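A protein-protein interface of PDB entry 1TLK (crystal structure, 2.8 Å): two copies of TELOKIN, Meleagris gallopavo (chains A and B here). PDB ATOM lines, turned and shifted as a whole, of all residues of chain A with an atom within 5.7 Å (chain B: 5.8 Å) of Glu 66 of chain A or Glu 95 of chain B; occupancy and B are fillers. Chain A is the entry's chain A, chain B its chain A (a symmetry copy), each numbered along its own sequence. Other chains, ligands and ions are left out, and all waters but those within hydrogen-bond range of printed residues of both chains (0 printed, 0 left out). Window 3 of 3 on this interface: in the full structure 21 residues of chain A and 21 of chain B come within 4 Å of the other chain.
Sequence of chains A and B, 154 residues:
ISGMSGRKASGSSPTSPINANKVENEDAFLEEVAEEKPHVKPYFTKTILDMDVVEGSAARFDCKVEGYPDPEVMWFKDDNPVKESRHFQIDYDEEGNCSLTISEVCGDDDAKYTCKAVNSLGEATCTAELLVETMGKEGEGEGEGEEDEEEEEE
Among the printed residues, pairs that only touch across the chains: Lys 37 of chain A with Asp 93 of chain B (3.0 Å).
The side-chain amino group (NZ) of Lys 37 of chain A sits close to the backbone carbonyl oxygen (O) of Glu 94 of chain B (3.3 Å).
The side-chain hydroxyl (OH) of Tyr 43 of chain A is in hydrogen-bond range of the side-chain carboxylate (OE1) of Glu 94 of chain B.
OE2 of Glu 66 of chain A sits close to OE2 of Glu 95 of chain B, at 3.2 Å.
The side-chain carboxylate (OE2) of Glu 66 of chain B lies close to the side-chain carboxylate (OE2) of Glu 95 of chain A (3.2 Å).
Glu 66 of chain A touches Glu 95 of chain B, and with the chains exchanged Glu 95 of chain A touches Glu 66 of chain B.
5 positions are printed for both chains.
Of the 5 pairs that touch across the chains among the printed residues, 2 have their exchanged pair printed and touching as well.
Of chain B, only Glu 95 comes within 4 Å of Glu 66 of chain A.
Glu 95 of chain B touches one residue of chain A.
Of the printed residues of chain B, Tyr 43 of chain A touches Glu 94 (2.5 Å).
Printed residues of chain A within 4 Å of Glu 66 of chain B: Glu 95 (3.2 Å).
Of the printed residues of chain A, Glu 94 of chain B touches Lys 37 (2.8 Å) and Tyr 43 (2.5 Å).
Of the printed residues of chain B, Glu 95 of chain A touches Glu 66 (3.2 Å).
Phe 44 of chain A touches none of the printed residues of chain B.
The nearest residue of chain A that does not touch Glu 95 of chain B is Thr 45 of chain A (4.2 Å).
The backbone NH (N) of Glu 66 of chain A lies within hydrogen-bond range of the backbone carbonyl oxygen (O) of Tyr 43 of chain A, 2.7 Å away.
The side-chain amino group (NZ) of Lys 64 of chain A lies within salt-bridge range of the side-chain carboxylate (OE1) of Glu 95 of chain A, 2.9 Å away.
The side-chain amino group (NZ) of Lys 64 of chain B lies within salt-bridge range of the side-chain carboxylate (OE1) of Glu 95 of chain B (2.9 Å).
The side-chain carboxylate (OD2) of Asp 93 of chain B lies close to the side-chain amide oxygen (OD1) of Asn 97 of chain B, 2.9 Å away.
Of the 8 printed residues of chain B, 4 touch a printed residue of chain A.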
ATOM      1  N   LYS A  37     -24.224  29.237   2.617  1.00  0.00           N
ATOM      2  CA  LYS A  37     -22.808  28.909   2.671  1.00  0.00           C
ATOM      3  C   LYS A  37     -22.081  29.373   1.424  1.00  0.00           C
ATOM      4  O   LYS A  37     -22.681  29.576   0.376  1.00  0.00           O
ATOM      5  CB  LYS A  37     -22.570  27.428   2.852  1.00  0.00           C
ATOM      6  CG  LYS A  37     -22.490  27.033   4.310  1.00  0.00           C
ATOM      7  CD  LYS A  37     -22.964  25.606   4.559  1.00  0.00           C
ATOM      8  CE  LYS A  37     -21.907  24.842   5.339  1.00  0.00           C
ATOM      9  NZ  LYS A  37     -22.469  23.664   6.119  1.00  0.00           N
ATOM     10  N   LYS A  41     -14.610  24.303  -3.328  1.00  0.00           N
ATOM     11  CA  LYS A  41     -14.280  22.978  -3.769  1.00  0.00           C
ATOM     12  C   LYS A  41     -13.940  22.068  -2.618  1.00  0.00           C
ATOM     13  O   LYS A  41     -13.554  22.514  -1.546  1.00  0.00           O
ATOM     14  CB  LYS A  41     -13.267  22.967  -4.883  1.00  0.00           C
ATOM     15  CG  LYS A  41     -12.076  23.865  -4.630  1.00  0.00           C
ATOM     16  CD  LYS A  41     -10.965  23.532  -5.604  1.00  0.00           C
ATOM     17  CE  LYS A  41      -9.595  23.468  -4.958  1.00  0.00           C
ATOM     18  NZ  LYS A  41      -8.590  22.834  -5.824  1.00  0.00           N
ATOM     19  N   PRO A  42     -14.098  20.788  -2.846  1.00  0.00           N
ATOM     20  CA  PRO A  42     -13.829  19.879  -1.780  1.00  0.00           C
ATOM     21  C   PRO A  42     -12.406  19.897  -1.289  1.00  0.00           C
ATOM     22  O   PRO A  42     -11.456  20.138  -2.031  1.00  0.00           O
ATOM     23  CB  PRO A  42     -14.246  18.494  -2.264  1.00  0.00           C
ATOM     24  CG  PRO A  42     -14.899  18.671  -3.628  1.00  0.00           C
ATOM     25  CD  PRO A  42     -14.687  20.116  -4.034  1.00  0.00           C
ATOM     26  N   TYR A  43     -12.301  19.621   0.001  1.00  0.00           N
ATOM     27  CA  TYR A  43     -11.033  19.544   0.697  1.00  0.00           C
ATOM     28  C   TYR A  43     -11.097  18.689   1.967  1.00  0.00           C
ATOM     29  O   TYR A  43     -12.133  18.640   2.633  1.00  0.00           O
ATOM     30  CB  TYR A  43     -10.374  20.912   0.921  1.00  0.00           C
ATOM     31  CG  TYR A  43     -11.025  21.798   1.964  1.00  0.00           C
ATOM     32  CD1 TYR A  43     -12.059  22.682   1.666  1.00  0.00           C
ATOM     33  CD2 TYR A  43     -10.590  21.791   3.286  1.00  0.00           C
ATOM     34  CE1 TYR A  43     -12.624  23.524   2.632  1.00  0.00           C
ATOM     35  CE2 TYR A  43     -11.186  22.583   4.274  1.00  0.00           C
ATOM     36  CZ  TYR A  43     -12.187  23.492   3.953  1.00  0.00           C
ATOM     37  OH  TYR A  43     -12.738  24.299   4.922  1.00  0.00           O
ATOM     38  N   PHE A  44      -9.997  17.965   2.268  1.00  0.00           N
ATOM     39  CA  PHE A  44      -9.825  17.079   3.425  1.00  0.00           C
ATOM     40  C   PHE A  44      -9.138  17.789   4.569  1.00  0.00           C
ATOM     41  O   PHE A  44      -8.021  18.279   4.420  1.00  0.00           O
ATOM     42  CB  PHE A  44      -8.943  15.860   3.092  1.00  0.00           C
ATOM     43  CG  PHE A  44      -9.687  14.887   2.235  1.00  0.00           C
ATOM     44  CD1 PHE A  44     -10.554  13.957   2.803  1.00  0.00           C
ATOM     45  CD2 PHE A  44      -9.524  14.910   0.849  1.00  0.00           C
ATOM     46  CE1 PHE A  44     -11.233  13.068   1.976  1.00  0.00           C
ATOM     47  CE2 PHE A  44     -10.181  14.024  -0.006  1.00  0.00           C
ATOM     48  CZ  PHE A  44     -11.091  13.153   0.591  1.00  0.00           C
ATOM     49  N   THR A  45      -9.809  17.824   5.707  1.00  0.00           N
ATOM     50  CA  THR A  45      -9.294  18.463   6.898  1.00  0.00           C
ATOM     51  C   THR A  45      -8.407  17.459   7.595  1.00  0.00           C
ATOM     52  O   THR A  45      -7.386  17.755   8.220  1.00  0.00           O
ATOM     53  CB  THR A  45     -10.547  19.044   7.590  1.00  0.00           C
ATOM     54  OG1 THR A  45     -10.776  20.404   7.295  1.00  0.00           O
ATOM     55  CG2 THR A  45     -10.858  18.645   9.032  1.00  0.00           C
ATOM     56  N   LYS A  64     -12.247  13.222   6.791  1.00  0.00           N
ATOM     57  CA  LYS A  64     -13.260  14.186   7.140  1.00  0.00           C
ATOM     58  C   LYS A  64     -13.310  15.151   5.976  1.00  0.00           C
ATOM     59  O   LYS A  64     -12.277  15.693   5.591  1.00  0.00           O
ATOM     60  CB  LYS A  64     -12.947  14.852   8.453  1.00  0.00           C
ATOM     61  CG  LYS A  64     -14.039  15.832   8.787  1.00  0.00           C
ATOM     62  CD  LYS A  64     -14.266  15.944  10.275  1.00  0.00           C
ATOM     63  CE  LYS A  64     -14.889  17.267  10.636  1.00  0.00           C
ATOM     64  NZ  LYS A  64     -15.137  17.372  12.095  1.00  0.00           N
ATOM     65  N   VAL A  65     -14.463  15.339   5.359  1.00  0.00           N
ATOM     66  CA  VAL A  65     -14.470  16.200   4.207  1.00  0.00           C
ATOM     67  C   VAL A  65     -15.179  17.490   4.338  1.00  0.00           C
ATOM     68  O   VAL A  65     -16.273  17.564   4.877  1.00  0.00           O
ATOM     69  CB  VAL A  65     -15.225  15.491   3.117  1.00  0.00           C
ATOM     70  CG1 VAL A  65     -15.156  16.282   1.817  1.00  0.00           C
ATOM     71  CG2 VAL A  65     -14.535  14.148   2.971  1.00  0.00           C
ATOM     72  N   GLU A  66     -14.562  18.503   3.773  1.00  0.00           N
ATOM     73  CA  GLU A  66     -15.166  19.808   3.784  1.00  0.00           C
ATOM     74  C   GLU A  66     -15.558  20.201   2.357  1.00  0.00           C
ATOM     75  O   GLU A  66     -15.159  19.543   1.400  1.00  0.00           O
ATOM     76  CB  GLU A  66     -14.285  20.869   4.468  1.00  0.00           C
ATOM     77  CG  GLU A  66     -13.997  20.581   5.957  1.00  0.00           C
ATOM     78  CD  GLU A  66     -15.211  20.567   6.845  1.00  0.00           C
ATOM     79  OE1 GLU A  66     -16.284  21.039   6.256  1.00  0.00           O
ATOM     80  OE2 GLU A  66     -15.195  20.147   7.987  1.00  0.00           O
ATOM     81  N   GLY A  67     -16.342  21.258   2.195  1.00  0.00           N
ATOM     82  CA  GLY A  67     -16.744  21.631   0.850  1.00  0.00           C
ATOM     83  C   GLY A  67     -18.234  21.887   0.778  1.00  0.00           C
ATOM     84  O   GLY A  67     -19.008  21.400   1.620  1.00  0.00           O
ATOM     85  N   TYR A  68     -18.632  22.621  -0.275  1.00  0.00           N
ATOM     86  CA  TYR A  68     -20.006  23.022  -0.554  1.00  0.00           C
ATOM     87  C   TYR A  68     -20.267  23.510  -1.966  1.00  0.00           C
ATOM     88  O   TYR A  68     -19.586  24.417  -2.441  1.00  0.00           O
ATOM     89  CB  TYR A  68     -20.306  24.298   0.230  1.00  0.00           C
ATOM     90  CG  TYR A  68     -21.738  24.689   0.009  1.00  0.00           C
ATOM     91  CD1 TYR A  68     -22.709  23.884   0.606  1.00  0.00           C
ATOM     92  CD2 TYR A  68     -22.130  25.834  -0.691  1.00  0.00           C
ATOM     93  CE1 TYR A  68     -24.063  24.165   0.429  1.00  0.00           C
ATOM     94  CE2 TYR A  68     -23.483  26.168  -0.776  1.00  0.00           C
ATOM     95  CZ  TYR A  68     -24.452  25.310  -0.264  1.00  0.00           C
ATOM     96  OH  TYR A  68     -25.779  25.627  -0.400  1.00  0.00           O
ATOM     97  N   PRO A  71     -19.746  17.596  -1.197  1.00  0.00           N
ATOM     98  CA  PRO A  71     -19.170  16.593  -2.085  1.00  0.00           C
ATOM     99  C   PRO A  71     -19.782  15.219  -2.043  1.00  0.00           C
ATOM    100  O   PRO A  71     -20.514  14.855  -1.131  1.00  0.00           O
ATOM    101  CB  PRO A  71     -17.718  16.384  -1.632  1.00  0.00           C
ATOM    102  CG  PRO A  71     -17.420  17.440  -0.580  1.00  0.00           C
ATOM    103  CD  PRO A  71     -18.737  18.125  -0.240  1.00  0.00           C
ATOM    104  N   GLU A  95     -21.462  15.898   9.148  1.00  0.00           N
ATOM    105  CA  GLU A  95     -20.295  16.690   9.502  1.00  0.00           C
ATOM    106  C   GLU A  95     -19.162  16.472   8.561  1.00  0.00           C
ATOM    107  O   GLU A  95     -18.120  17.110   8.685  1.00  0.00           O
ATOM    108  CB  GLU A  95     -19.764  16.513  10.924  1.00  0.00           C
ATOM    109  CG  GLU A  95     -20.193  17.671  11.823  1.00  0.00           C
ATOM    110  CD  GLU A  95     -19.210  17.887  12.924  1.00  0.00           C
ATOM    111  OE1 GLU A  95     -18.022  17.411  12.644  1.00  0.00           O
ATOM    112  OE2 GLU A  95     -19.497  18.426  13.973  1.00  0.00           O
ATOM    113  N   GLY A  96     -19.357  15.550   7.641  1.00  0.00           N
ATOM    114  CA  GLY A  96     -18.303  15.290   6.687  1.00  0.00           C
ATOM    115  C   GLY A  96     -17.356  14.190   7.112  1.00  0.00           C
ATOM    116  O   GLY A  96     -16.366  13.879   6.447  1.00  0.00           O
ATOM    117  N   LYS B  64     -21.810  27.824  15.492  1.00  0.00           N
ATOM    118  CA  LYS B  64     -21.321  26.899  14.499  1.00  0.00           C
ATOM    119  C   LYS B  64     -22.508  26.028  14.149  1.00  0.00           C
ATOM    120  O   LYS B  64     -23.126  25.454  15.042  1.00  0.00           O
ATOM    121  CB  LYS B  64     -20.142  26.120  15.016  1.00  0.00           C
ATOM    122  CG  LYS B  64     -19.653  25.186  13.943  1.00  0.00           C
ATOM    123  CD  LYS B  64     -18.159  24.979  14.008  1.00  0.00           C
ATOM    124  CE  LYS B  64     -17.760  23.673  13.372  1.00  0.00           C
ATOM    125  NZ  LYS B  64     -16.290  23.475  13.411  1.00  0.00           N
ATOM    126  N   VAL B  65     -22.888  25.955  12.886  1.00  0.00           N
ATOM    127  CA  VAL B  65     -24.065  25.183  12.587  1.00  0.00           C
ATOM    128  C   VAL B  65     -23.870  23.931  11.825  1.00  0.00           C
ATOM    129  O   VAL B  65     -23.127  23.884  10.857  1.00  0.00           O
ATOM    130  CB  VAL B  65     -24.934  26.014  11.686  1.00  0.00           C
ATOM    131  CG1 VAL B  65     -26.267  25.319  11.438  1.00  0.00           C
ATOM    132  CG2 VAL B  65     -25.136  27.321  12.431  1.00  0.00           C
ATOM    133  N   GLU B  66     -24.608  22.928  12.242  1.00  0.00           N
ATOM    134  CA  GLU B  66     -24.554  21.665  11.557  1.00  0.00           C
ATOM    135  C   GLU B  66     -25.892  21.402  10.863  1.00  0.00           C
ATOM    136  O   GLU B  66     -26.870  22.103  11.112  1.00  0.00           O
ATOM    137  CB  GLU B  66     -24.127  20.505  12.476  1.00  0.00           C
ATOM    138  CG  GLU B  66     -22.713  20.664  13.073  1.00  0.00           C
ATOM    139  CD  GLU B  66     -21.598  20.686  12.064  1.00  0.00           C
ATOM    140  OE1 GLU B  66     -21.985  20.324  10.864  1.00  0.00           O
ATOM    141  OE2 GLU B  66     -20.460  21.019  12.337  1.00  0.00           O
ATOM    142  N   ASP B  93     -19.127  30.253   7.151  1.00  0.00           N
ATOM    143  CA  ASP B  93     -18.302  29.282   6.452  1.00  0.00           C
ATOM    144  C   ASP B  93     -18.996  28.146   5.817  1.00  0.00           C
ATOM    145  O   ASP B  93     -20.180  27.902   6.041  1.00  0.00           O
ATOM    146  CB  ASP B  93     -17.699  28.380   7.518  1.00  0.00           C
ATOM    147  CG  ASP B  93     -16.464  28.958   8.060  1.00  0.00           C
ATOM    148  OD1 ASP B  93     -16.301  30.200   7.685  1.00  0.00           O
ATOM    149  OD2 ASP B  93     -15.700  28.338   8.769  1.00  0.00           O
ATOM    150  N   GLU B  94     -18.153  27.405   5.128  1.00  0.00           N
ATOM    151  CA  GLU B  94     -18.548  26.181   4.527  1.00  0.00           C
ATOM    152  C   GLU B  94     -18.553  25.201   5.700  1.00  0.00           C
ATOM    153  O   GLU B  94     -19.188  24.149   5.666  1.00  0.00           O
ATOM    154  CB  GLU B  94     -17.428  25.739   3.579  1.00  0.00           C
ATOM    155  CG  GLU B  94     -16.516  26.924   3.198  1.00  0.00           C
ATOM    156  CD  GLU B  94     -15.091  26.753   3.630  1.00  0.00           C
ATOM    157  OE1 GLU B  94     -14.610  25.686   3.964  1.00  0.00           O
ATOM    158  OE2 GLU B  94     -14.417  27.879   3.608  1.00  0.00           O
ATOM    159  N   GLU B  95     -17.800  25.540   6.754  1.00  0.00           N
ATOM    160  CA  GLU B  95     -17.739  24.655   7.906  1.00  0.00           C
ATOM    161  C   GLU B  95     -18.875  24.874   8.843  1.00  0.00           C
ATOM    162  O   GLU B  95     -19.003  24.167   9.839  1.00  0.00           O
ATOM    163  CB  GLU B  95     -16.446  24.695   8.719  1.00  0.00           C
ATOM    164  CG  GLU B  95     -15.550  23.502   8.392  1.00  0.00           C
ATOM    165  CD  GLU B  95     -14.685  23.147   9.556  1.00  0.00           C
ATOM    166  OE1 GLU B  95     -15.171  23.569  10.697  1.00  0.00           O
ATOM    167  OE2 GLU B  95     -13.634  22.549   9.444  1.00  0.00           O
ATOM    168  N   GLY B  96     -19.680  25.871   8.539  1.00  0.00           N
ATOM    169  CA  GLY B  96     -20.810  26.137   9.399  1.00  0.00           C
ATOM    170  C   GLY B  96     -20.519  27.143  10.490  1.00  0.00           C
ATOM    171  O   GLY B  96     -21.352  27.443  11.349  1.00  0.00           O
ATOM    172  N   ASN B  97     -19.304  27.634  10.431  1.00  0.00           N
ATOM    173  CA  ASN B  97     -18.918  28.623  11.383  1.00  0.00           C
ATOM    174  C   ASN B  97     -19.724  29.838  10.959  1.00  0.00           C
ATOM    175  O   ASN B  97     -19.625  30.280   9.817  1.00  0.00           O
ATOM    176  CB  ASN B  97     -17.403  28.870  11.300  1.00  0.00           C
ATOM    177  CG  ASN B  97     -16.576  27.811  11.998  1.00  0.00           C
ATOM    178  OD1 ASN B  97     -15.714  27.175  11.373  1.00  0.00           O
ATOM    179  ND2 ASN B  97     -16.797  27.650  13.300  1.00  0.00           N
